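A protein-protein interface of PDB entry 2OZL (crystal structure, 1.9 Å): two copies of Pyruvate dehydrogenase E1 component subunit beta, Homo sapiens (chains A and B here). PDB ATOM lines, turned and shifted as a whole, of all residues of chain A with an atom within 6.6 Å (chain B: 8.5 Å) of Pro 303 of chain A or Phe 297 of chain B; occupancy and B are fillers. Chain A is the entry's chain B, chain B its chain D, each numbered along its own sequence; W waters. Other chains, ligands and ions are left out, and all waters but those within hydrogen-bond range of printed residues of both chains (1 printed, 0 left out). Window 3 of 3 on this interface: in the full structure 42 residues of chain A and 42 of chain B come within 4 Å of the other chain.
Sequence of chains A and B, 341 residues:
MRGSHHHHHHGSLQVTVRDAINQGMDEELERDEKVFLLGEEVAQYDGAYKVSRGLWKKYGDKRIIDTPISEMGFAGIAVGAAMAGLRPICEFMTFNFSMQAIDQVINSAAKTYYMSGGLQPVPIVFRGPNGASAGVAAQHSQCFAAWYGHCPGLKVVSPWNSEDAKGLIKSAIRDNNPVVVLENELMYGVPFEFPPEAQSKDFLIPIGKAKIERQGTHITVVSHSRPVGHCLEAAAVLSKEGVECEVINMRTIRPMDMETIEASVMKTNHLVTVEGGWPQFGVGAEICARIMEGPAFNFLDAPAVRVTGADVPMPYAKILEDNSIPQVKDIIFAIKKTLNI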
ATOM      1  N   HIS A 270      12.472  26.136 -13.419  1.00  0.00           N
ATOM      2  CA  HIS A 270      13.217  26.920 -14.407  1.00  0.00           C
ATOM      3  C   HIS A 270      12.990  28.417 -14.217  1.00  0.00           C
ATOM      4  O   HIS A 270      11.940  28.836 -13.722  1.00  0.00           O
ATOM      5  CB  HIS A 270      12.822  26.524 -15.834  1.00  0.00           C
ATOM      6  CG  HIS A 270      13.011  25.069 -16.130  1.00  0.00           C
ATOM      7  ND1 HIS A 270      12.119  24.103 -15.714  1.00  0.00           N
ATOM      8  CD2 HIS A 270      14.004  24.411 -16.776  1.00  0.00           C
ATOM      9  CE1 HIS A 270      12.555  22.913 -16.093  1.00  0.00           C
ATOM     10  NE2 HIS A 270      13.697  23.073 -16.738  1.00  0.00           N
ATOM     11  N   LEU A 271      13.970  29.218 -14.626  1.00  0.00           N
ATOM     12  CA  LEU A 271      13.883  30.669 -14.477  1.00  0.00           C
ATOM     13  C   LEU A 271      14.600  31.470 -15.557  1.00  0.00           C
ATOM     14  O   LEU A 271      15.708  31.141 -15.972  1.00  0.00           O
ATOM     15  CB  LEU A 271      14.453  31.086 -13.115  1.00  0.00           C
ATOM     16  CG  LEU A 271      14.566  32.586 -12.811  1.00  0.00           C
ATOM     17  CD1 LEU A 271      13.185  33.179 -12.640  1.00  0.00           C
ATOM     18  CD2 LEU A 271      15.390  32.793 -11.539  1.00  0.00           C
ATOM     19  N   VAL A 272      13.948  32.538 -15.992  1.00  0.00           N
ATOM     20  CA  VAL A 272      14.502  33.448 -16.980  1.00  0.00           C
ATOM     21  C   VAL A 272      14.129  34.837 -16.470  1.00  0.00           C
ATOM     22  O   VAL A 272      13.000  35.054 -16.026  1.00  0.00           O
ATOM     23  CB  VAL A 272      13.874  33.229 -18.382  1.00  0.00           C
ATOM     24  CG1 VAL A 272      14.332  34.321 -19.346  1.00  0.00           C
ATOM     25  CG2 VAL A 272      14.275  31.862 -18.922  1.00  0.00           C
ATOM     26  N   MET A 292      20.465  31.339  -6.494  1.00  0.00           N
ATOM     27  CA  MET A 292      21.515  30.367  -6.217  1.00  0.00           C
ATOM     28  C   MET A 292      21.841  30.271  -4.731  1.00  0.00           C
ATOM     29  O   MET A 292      22.223  29.206  -4.248  1.00  0.00           O
ATOM     30  CB  MET A 292      22.787  30.695  -7.018  1.00  0.00           C
ATOM     31  CG  MET A 292      23.905  29.651  -6.873  1.00  0.00           C
ATOM     32  SD  MET A 292      25.046  29.594  -8.295  1.00  0.00           S
ATOM     33  CE  MET A 292      25.613  31.293  -8.336  1.00  0.00           C
ATOM     34  N   PHE A 297      17.317  26.914  -5.059  1.00  0.00           N
ATOM     35  CA  PHE A 297      18.389  26.419  -5.917  1.00  0.00           C
ATOM     36  C   PHE A 297      18.304  24.920  -6.190  1.00  0.00           C
ATOM     37  O   PHE A 297      18.539  24.486  -7.317  1.00  0.00           O
ATOM     38  CB  PHE A 297      19.764  26.753  -5.327  1.00  0.00           C
ATOM     39  CG  PHE A 297      20.916  26.413  -6.243  1.00  0.00           C
ATOM     40  CD1 PHE A 297      21.041  27.033  -7.486  1.00  0.00           C
ATOM     41  CD2 PHE A 297      21.878  25.481  -5.861  1.00  0.00           C
ATOM     42  CE1 PHE A 297      22.110  26.730  -8.336  1.00  0.00           C
ATOM     43  CE2 PHE A 297      22.951  25.169  -6.702  1.00  0.00           C
ATOM     44  CZ  PHE A 297      23.067  25.796  -7.944  1.00  0.00           C
ATOM     45  N   LEU A 300      15.976  24.019  -9.075  1.00  0.00           N
ATOM     46  CA  LEU A 300      16.327  24.490 -10.405  1.00  0.00           C
ATOM     47  C   LEU A 300      16.910  23.330 -11.218  1.00  0.00           C
ATOM     48  O   LEU A 300      17.951  22.780 -10.860  1.00  0.00           O
ATOM     49  CB  LEU A 300      17.348  25.620 -10.265  1.00  0.00           C
ATOM     50  CG  LEU A 300      17.449  26.716 -11.324  1.00  0.00           C
ATOM     51  CD1 LEU A 300      16.100  27.387 -11.523  1.00  0.00           C
ATOM     52  CD2 LEU A 300      18.493  27.731 -10.874  1.00  0.00           C
ATOM     53  N   ASP A 301      16.235  22.953 -12.302  1.00  0.00           N
ATOM     54  CA  ASP A 301      16.699  21.851 -13.147  1.00  0.00           C
ATOM     55  C   ASP A 301      17.620  22.316 -14.281  1.00  0.00           C
ATOM     56  O   ASP A 301      18.264  21.503 -14.950  1.00  0.00           O
ATOM     57  CB  ASP A 301      15.498  21.088 -13.719  1.00  0.00           C
ATOM     58  CG  ASP A 301      14.753  20.285 -12.656  1.00  0.00           C
ATOM     59  OD1 ASP A 301      13.632  19.804 -12.940  1.00  0.00           O
ATOM     60  OD2 ASP A 301      15.289  20.128 -11.536  1.00  0.00           O
ATOM     61  N   ALA A 302      17.681  23.626 -14.492  1.00  0.00           N
ATOM     62  CA  ALA A 302      18.530  24.206 -15.529  1.00  0.00           C
ATOM     63  C   ALA A 302      18.975  25.574 -15.035  1.00  0.00           C
ATOM     64  O   ALA A 302      18.245  26.239 -14.304  1.00  0.00           O
ATOM     65  CB  ALA A 302      17.753  24.345 -16.831  1.00  0.00           C
ATOM     66  N   PRO A 303      20.178  26.017 -15.424  1.00  0.00           N
ATOM     67  CA  PRO A 303      20.634  27.331 -14.962  1.00  0.00           C
ATOM     68  C   PRO A 303      19.721  28.468 -15.403  1.00  0.00           C
ATOM     69  O   PRO A 303      19.087  28.400 -16.458  1.00  0.00           O
ATOM     70  CB  PRO A 303      22.035  27.442 -15.558  1.00  0.00           C
ATOM     71  CG  PRO A 303      21.923  26.645 -16.826  1.00  0.00           C
ATOM     72  CD  PRO A 303      21.140  25.429 -16.372  1.00  0.00           C
ATOM     73  N   ALA A 304      19.640  29.504 -14.576  1.00  0.00           N
ATOM     74  CA  ALA A 304      18.816  30.657 -14.905  1.00  0.00           C
ATOM     75  C   ALA A 304      19.578  31.475 -15.946  1.00  0.00           C
ATOM     76  O   ALA A 304      20.805  31.576 -15.889  1.00  0.00           O
ATOM     77  CB  ALA A 304      18.558  31.496 -13.656  1.00  0.00           C
ATOM     78  N   VAL A 305      18.856  32.037 -16.908  1.00  0.00           N
ATOM     79  CA  VAL A 305      19.479  32.850 -17.945  1.00  0.00           C
ATOM     80  C   VAL A 305      18.872  34.249 -17.932  1.00  0.00           C
ATOM     81  O   VAL A 305      17.757  34.445 -17.445  1.00  0.00           O
ATOM     82  CB  VAL A 305      19.294  32.222 -19.341  1.00  0.00           C
ATOM     83  CG1 VAL A 305      20.059  30.901 -19.416  1.00  0.00           C
ATOM     84  CG2 VAL A 305      17.827  31.999 -19.617  1.00  0.00           C
ATOM     85  N   THR A 338      16.410  27.359 -22.287  1.00  0.00           N
ATOM     86  CA  THR A 338      16.329  26.938 -20.891  1.00  0.00           C
ATOM     87  C   THR A 338      15.599  25.606 -20.716  1.00  0.00           C
ATOM     88  O   THR A 338      15.945  24.807 -19.845  1.00  0.00           O
ATOM     89  CB  THR A 338      15.607  28.003 -20.030  1.00  0.00           C
ATOM     90  OG1 THR A 338      16.335  29.233 -20.090  1.00  0.00           O
ATOM     91  CG2 THR A 338      15.518  27.553 -18.579  1.00  0.00           C
ATOM     92  N   MET B 258      36.386  36.900 -16.765  1.00  0.00           N
ATOM     93  CA  MET B 258      35.591  35.752 -16.363  1.00  0.00           C
ATOM     94  C   MET B 258      36.270  34.438 -16.763  1.00  0.00           C
ATOM     95  O   MET B 258      36.081  33.413 -16.109  1.00  0.00           O
ATOM     96  CB  MET B 258      34.204  35.850 -17.000  1.00  0.00           C
ATOM     97  CG  MET B 258      33.117  35.095 -16.263  1.00  0.00           C
ATOM     98  SD  MET B 258      32.865  35.670 -14.556  1.00  0.00           S
ATOM     99  CE  MET B 258      32.643  34.103 -13.759  1.00  0.00           C
ATOM    100  N   GLU B 262      36.405  31.166 -14.417  1.00  0.00           N
ATOM    101  CA  GLU B 262      35.775  29.925 -14.852  1.00  0.00           C
ATOM    102  C   GLU B 262      36.779  28.774 -14.908  1.00  0.00           C
ATOM    103  O   GLU B 262      36.452  27.643 -14.551  1.00  0.00           O
ATOM    104  CB  GLU B 262      35.106  30.121 -16.220  1.00  0.00           C
ATOM    105  CG  GLU B 262      34.000  31.180 -16.203  1.00  0.00           C
ATOM    106  CD  GLU B 262      33.298  31.356 -17.544  1.00  0.00           C
ATOM    107  OE1 GLU B 262      33.994  31.417 -18.581  1.00  0.00           O
ATOM    108  OE2 GLU B 262      32.048  31.451 -17.558  1.00  0.00           O
ATOM    109  N   VAL B 265      37.232  27.578 -11.357  1.00  0.00           N
ATOM    110  CA  VAL B 265      36.074  26.836 -10.866  1.00  0.00           C
ATOM    111  C   VAL B 265      36.029  25.432 -11.474  1.00  0.00           C
ATOM    112  O   VAL B 265      35.560  24.489 -10.838  1.00  0.00           O
ATOM    113  CB  VAL B 265      34.759  27.576 -11.199  1.00  0.00           C
ATOM    114  CG1 VAL B 265      33.559  26.667 -10.943  1.00  0.00           C
ATOM    115  CG2 VAL B 265      34.650  28.841 -10.350  1.00  0.00           C
ATOM    116  N   MET B 266      36.517  25.297 -12.703  1.00  0.00           N
ATOM    117  CA  MET B 266      36.531  23.998 -13.368  1.00  0.00           C
ATOM    118  C   MET B 266      37.486  23.047 -12.655  1.00  0.00           C
ATOM    119  O   MET B 266      37.438  21.832 -12.852  1.00  0.00           O
ATOM    120  CB  MET B 266      36.952  24.149 -14.829  1.00  0.00           C
ATOM    121  CG  MET B 266      35.943  24.893 -15.678  1.00  0.00           C
ATOM    122  SD  MET B 266      36.475  25.035 -17.394  1.00  0.00           S
ATOM    123  CE  MET B 266      34.933  25.490 -18.180  1.00  0.00           C
ATOM    124  N   ASN B 269      35.575  23.363  -8.262  1.00  0.00           N
ATOM    125  CA  ASN B 269      34.161  23.013  -8.121  1.00  0.00           C
ATOM    126  C   ASN B 269      33.431  23.829  -7.055  1.00  0.00           C
ATOM    127  O   ASN B 269      32.295  23.514  -6.705  1.00  0.00           O
ATOM    128  CB  ASN B 269      33.996  21.524  -7.798  1.00  0.00           C
ATOM    129  CG  ASN B 269      34.907  20.646  -8.622  1.00  0.00           C
ATOM    130  OD1 ASN B 269      35.927  20.170  -8.134  1.00  0.00           O
ATOM    131  ND2 ASN B 269      34.550  20.435  -9.883  1.00  0.00           N
ATOM    132  N   CYS B 288      28.392  35.739  -9.990  1.00  0.00           N
ATOM    133  CA  CYS B 288      27.557  34.565  -9.770  1.00  0.00           C
ATOM    134  C   CYS B 288      26.629  34.297 -10.955  1.00  0.00           C
ATOM    135  O   CYS B 288      26.433  33.147 -11.349  1.00  0.00           O
ATOM    136  CB  CYS B 288      26.740  34.729  -8.482  1.00  0.00           C
ATOM    137  SG  CYS B 288      27.731  34.564  -6.969  1.00  0.00           S
ATOM    138  N   ALA B 289      26.064  35.356 -11.524  1.00  0.00           N
ATOM    139  CA  ALA B 289      25.171  35.201 -12.665  1.00  0.00           C
ATOM    140  C   ALA B 289      25.945  34.717 -13.891  1.00  0.00           C
ATOM    141  O   ALA B 289      25.444  33.901 -14.663  1.00  0.00           O
ATOM    142  CB  ALA B 289      24.462  36.527 -12.967  1.00  0.00           C
ATOM    143  N   ARG B 290      27.163  35.222 -14.065  1.00  0.00           N
ATOM    144  CA  ARG B 290      28.009  34.836 -15.192  1.00  0.00           C
ATOM    145  C   ARG B 290      28.449  33.382 -15.050  1.00  0.00           C
ATOM    146  O   ARG B 290      28.612  32.673 -16.040  1.00  0.00           O
ATOM    147  CB  ARG B 290      29.249  35.736 -15.259  1.00  0.00           C
ATOM    148  CG  ARG B 290      28.930  37.184 -15.571  1.00  0.00           C
ATOM    149  CD  ARG B 290      28.673  37.368 -17.042  1.00  0.00           C
ATOM    150  NE  ARG B 290      29.922  37.589 -17.764  1.00  0.00           N
ATOM    151  CZ  ARG B 290      30.595  38.738 -17.754  1.00  0.00           C
ATOM    152  NH1 ARG B 290      30.137  39.779 -17.062  1.00  0.00           N
ATOM    153  NH2 ARG B 290      31.728  38.842 -18.433  1.00  0.00           N
ATOM    154  N   ILE B 291      28.664  32.947 -13.815  1.00  0.00           N
ATOM    155  CA  ILE B 291      29.068  31.570 -13.580  1.00  0.00           C
ATOM    156  C   ILE B 291      27.927  30.631 -13.954  1.00  0.00           C
ATOM    157  O   ILE B 291      28.153  29.571 -14.544  1.00  0.00           O
ATOM    158  CB  ILE B 291      29.462  31.342 -12.101  1.00  0.00           C
ATOM    159  CG1 ILE B 291      30.875  31.870 -11.859  1.00  0.00           C
ATOM    160  CG2 ILE B 291      29.414  29.863 -11.764  1.00  0.00           C
ATOM    161  CD1 ILE B 291      31.949  31.119 -12.648  1.00  0.00           C
ATOM    162  N   MET B 292      26.701  31.032 -13.631  1.00  0.00           N
ATOM    163  CA  MET B 292      25.533  30.208 -13.932  1.00  0.00           C
ATOM    164  C   MET B 292      25.197  30.193 -15.422  1.00  0.00           C
ATOM    165  O   MET B 292      24.561  29.255 -15.908  1.00  0.00           O
ATOM    166  CB  MET B 292      24.319  30.682 -13.125  1.00  0.00           C
ATOM    167  CG  MET B 292      23.154  29.705 -13.167  1.00  0.00           C
ATOM    168  SD  MET B 292      21.888  30.035 -11.928  1.00  0.00           S
ATOM    169  CE  MET B 292      22.631  29.335 -10.486  1.00  0.00           C
ATOM    170  N   GLU B 293      25.622  31.225 -16.147  1.00  0.00           N
ATOM    171  CA  GLU B 293      25.366  31.295 -17.586  1.00  0.00           C
ATOM    172  C   GLU B 293      26.517  30.677 -18.378  1.00  0.00           C
ATOM    173  O   GLU B 293      26.351  30.331 -19.547  1.00  0.00           O
ATOM    174  CB  GLU B 293      25.222  32.745 -18.060  1.00  0.00           C
ATOM    175  CG  GLU B 293      24.078  33.531 -17.471  1.00  0.00           C
ATOM    176  CD  GLU B 293      24.005  34.932 -18.057  1.00  0.00           C
ATOM    177  OE1 GLU B 293      25.047  35.616 -18.079  1.00  0.00           O
ATOM    178  OE2 GLU B 293      22.911  35.346 -18.496  1.00  0.00           O
ATOM    179  N   GLY B 294      27.681  30.555 -17.745  1.00  0.00           N
ATOM    180  CA  GLY B 294      28.845  30.024 -18.436  1.00  0.00           C
ATOM    181  C   GLY B 294      29.060  28.521 -18.439  1.00  0.00           C
ATOM    182  O   GLY B 294      28.244  27.764 -17.912  1.00  0.00           O
ATOM    183  N   PRO B 295      30.172  28.060 -19.039  1.00  0.00           N
ATOM    184  CA  PRO B 295      30.512  26.636 -19.120  1.00  0.00           C
ATOM    185  C   PRO B 295      30.989  26.036 -17.801  1.00  0.00           C
ATOM    186  O   PRO B 295      31.100  24.820 -17.675  1.00  0.00           O
ATOM    187  CB  PRO B 295      31.594  26.604 -20.195  1.00  0.00           C
ATOM    188  CG  PRO B 295      32.303  27.910 -19.978  1.00  0.00           C
ATOM    189  CD  PRO B 295      31.152  28.877 -19.781  1.00  0.00           C
ATOM    190  N   ALA B 296      31.259  26.883 -16.816  1.00  0.00           N
ATOM    191  CA  ALA B 296      31.732  26.401 -15.524  1.00  0.00           C
ATOM    192  C   ALA B 296      30.600  26.000 -14.576  1.00  0.00           C
ATOM    193  O   ALA B 296      30.838  25.330 -13.570  1.00  0.00           O
ATOM    194  CB  ALA B 296      32.615  27.458 -14.866  1.00  0.00           C
ATOM    195  N   PHE B 297      29.369  26.392 -14.896  1.00  0.00           N
ATOM    196  CA  PHE B 297      28.241  26.066 -14.033  1.00  0.00           C
ATOM    197  C   PHE B 297      28.131  24.588 -13.665  1.00  0.00           C
ATOM    198  O   PHE B 297      27.899  24.253 -12.503  1.00  0.00           O
ATOM    199  CB  PHE B 297      26.924  26.501 -14.665  1.00  0.00           C
ATOM    200  CG  PHE B 297      25.727  26.228 -13.796  1.00  0.00           C
ATOM    201  CD1 PHE B 297      25.553  26.915 -12.597  1.00  0.00           C
ATOM    202  CD2 PHE B 297      24.791  25.263 -14.157  1.00  0.00           C
ATOM    203  CE1 PHE B 297      24.463  26.647 -11.770  1.00  0.00           C
ATOM    204  CE2 PHE B 297      23.698  24.985 -13.337  1.00  0.00           C
ATOM    205  CZ  PHE B 297      23.534  25.679 -12.140  1.00  0.00           C
ATOM    206  N   ASN B 298      28.282  23.704 -14.648  1.00  0.00           N
ATOM    207  CA  ASN B 298      28.175  22.271 -14.385  1.00  0.00           C
ATOM    208  C   ASN B 298      29.328  21.717 -13.555  1.00  0.00           C
ATOM    209  O   ASN B 298      29.252  20.592 -13.063  1.00  0.00           O
ATOM    210  CB  ASN B 298      28.070  21.481 -15.694  1.00  0.00           C
ATOM    211  CG  ASN B 298      26.720  21.646 -16.369  1.00  0.00           C
ATOM    212  OD1 ASN B 298      25.678  21.631 -15.713  1.00  0.00           O
ATOM    213  ND2 ASN B 298      26.733  21.788 -17.688  1.00  0.00           N
ATOM    214  N   PHE B 299      30.391  22.499 -13.403  1.00  0.00           N
ATOM    215  CA  PHE B 299      31.552  22.071 -12.624  1.00  0.00           C
ATOM    216  C   PHE B 299      31.379  22.372 -11.132  1.00  0.00           C
ATOM    217  O   PHE B 299      32.204  21.979 -10.310  1.00  0.00           O
ATOM    218  CB  PHE B 299      32.819  22.759 -13.146  1.00  0.00           C
ATOM    219  CG  PHE B 299      33.283  22.249 -14.484  1.00  0.00           C
ATOM    220  CD1 PHE B 299      34.284  21.284 -14.567  1.00  0.00           C
ATOM    221  CD2 PHE B 299      32.718  22.726 -15.661  1.00  0.00           C
ATOM    222  CE1 PHE B 299      34.715  20.804 -15.799  1.00  0.00           C
ATOM    223  CE2 PHE B 299      33.139  22.252 -16.906  1.00  0.00           C
ATOM    224  CZ  PHE B 299      34.141  21.288 -16.975  1.00  0.00           C
ATOM    225  N   LEU B 300      30.302  23.069 -10.792  1.00  0.00           N
ATOM    226  CA  LEU B 300      30.014  23.428  -9.408  1.00  0.00           C
ATOM    227  C   LEU B 300      29.500  22.229  -8.614  1.00  0.00           C
ATOM    228  O   LEU B 300      28.704  21.438  -9.117  1.00  0.00           O
ATOM    229  CB  LEU B 300      28.967  24.550  -9.380  1.00  0.00           C
ATOM    230  CG  LEU B 300      29.322  25.947  -8.861  1.00  0.00           C
ATOM    231  CD1 LEU B 300      30.738  26.327  -9.215  1.00  0.00           C
ATOM    232  CD2 LEU B 300      28.330  26.943  -9.435  1.00  0.00           C
ATOM    233  N   ASP B 301      29.972  22.083  -7.380  1.00  0.00           N
ATOM    234  CA  ASP B 301      29.525  20.997  -6.515  1.00  0.00           C
ATOM    235  C   ASP B 301      28.635  21.591  -5.424  1.00  0.00           C
ATOM    236  O   ASP B 301      27.987  20.871  -4.666  1.00  0.00           O
ATOM    237  CB  ASP B 301      30.724  20.282  -5.880  1.00  0.00           C
ATOM    238  CG  ASP B 301      31.389  19.289  -6.827  1.00  0.00           C
ATOM    239  OD1 ASP B 301      32.410  18.689  -6.430  1.00  0.00           O
ATOM    240  OD2 ASP B 301      30.894  19.098  -7.960  1.00  0.00           O
ATOM    241  N   ALA B 302      28.613  22.917  -5.355  1.00  0.00           N
ATOM    242  CA  ALA B 302      27.807  23.636  -4.373  1.00  0.00           C
ATOM    243  C   ALA B 302      27.487  25.006  -4.947  1.00  0.00           C
ATOM    244  O   ALA B 302      28.225  25.518  -5.786  1.00  0.00           O
ATOM    245  CB  ALA B 302      28.577  23.786  -3.069  1.00  0.00           C
ATOM    246  N   PRO B 303      26.380  25.618  -4.510  1.00  0.00           N
ATOM    247  CA  PRO B 303      26.038  26.939  -5.039  1.00  0.00           C
ATOM    248  C   PRO B 303      27.084  27.984  -4.676  1.00  0.00           C
ATOM    249  O   PRO B 303      27.705  27.909  -3.618  1.00  0.00           O
ATOM    250  CB  PRO B 303      24.678  27.225  -4.401  1.00  0.00           C
ATOM    251  CG  PRO B 303      24.764  26.503  -3.086  1.00  0.00           C
ATOM    252  CD  PRO B 303      25.414  25.192  -3.482  1.00  0.00           C
ATOM    253  N   ALA B 304      27.298  28.943  -5.570  1.00  0.00           N
ATOM    254  CA  ALA B 304      28.259  30.006  -5.306  1.00  0.00           C
ATOM    255  C   ALA B 304      27.602  30.938  -4.297  1.00  0.00           C
ATOM    256  O   ALA B 304      26.402  31.196  -4.380  1.00  0.00           O
ATOM    257  CB  ALA B 304      28.575  30.764  -6.589  1.00  0.00           C
HETATM  258  O   HOH W   1      22.193  30.131 -17.601  1.00  0.00           O
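The backbone NH (N) of Ala 304 of chain A is in hydrogen-bond range of the side-chain sulfur (SD) of Met 292 of chain B, at 3.5 Å.
The backbone NH of Ala 304 of chain B lies within hydrogen-bond range of the side-chain sulfur of Met 292 of chain A, at 3.6 Å.
The backbone NH (N) of Phe 297 of chain B sits close to the backbone carbonyl oxygen (O) of Ile 291 of chain B (3.4 Å).
CE of Met 292 of chain A touches CB of Cys 288 of chain B, at 3.6 Å.
Met 292 of chain B touches Met 292 of chain A (CE to SD, 3.3 Å).
Met 292 of chain A touches Pro 303 of chain B.
CE1 of Phe 297 of chain A touches CE of Met 292 of chain B (3.4 Å).
CB of Pro 303 of chain B touches CE2 of Phe 297 of chain A, at 3.5 Å.
Pro 303 of chain A touches Met 292 of chain B.
Pro 303 of chain A touches Phe 297 of chain B.
Leu 300 of chain A touches none of the printed residues of chain B.
No residue of chain B comes within 4 Å of Ala 302 of chain A.
Of the printed residues of chain B, Ala 304 of chain A touches Met 292 (3.5 Å).
Of the printed residues of chain A, Cys 288 of chain B touches Met 292.
Of the printed residues of chain A, Ala 304 of chain B touches Met 292.
The nearest residue of chain B that does not touch Pro 303 of chain A is Glu 293 of chain B (5.2 Å).
The nearest printed residue of chain B that does not touch Met 292 of chain A is Leu 300 of chain B (4.4 Å).
Of the 12 printed residues of chain A, 4 touch a printed residue of chain B.
Hydrophobic or aromatic side chains of chain A that line the printed part of chain B: Met 292, Phe 297 and Pro 303.
Among the printed residues, no Asp or Glu carboxylate lies within 4 Å of a Lys or Arg side-chain nitrogen of the other chain.
Met 292 of chain A touches its own counterpart, Met 292 of chain B.
Met 292 of chain A touches Ala 304 of chain B, and with the chains exchanged Ala 304 of chain A touches Met 292 of chain B.
Phe 297 of chain A touches Met 292 of chain B, but with the chains exchanged Met 292 of chain A does not touch Phe 297 of chain B (4.6 Å).
Phe 297 of chain A touches Pro 303 of chain B, and with the chains exchanged Pro 303 of chain A touches Phe 297 of chain B.
7 positions are printed for both chains.
Of the 9 pairs that touch across the chains among the printed residues, 7 have their exchanged pair printed and touching as well.
Water W1 bridges O of Ala 304 of chain A (2.6 Å) and O of Met 292 of chain B (3.0 Å).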
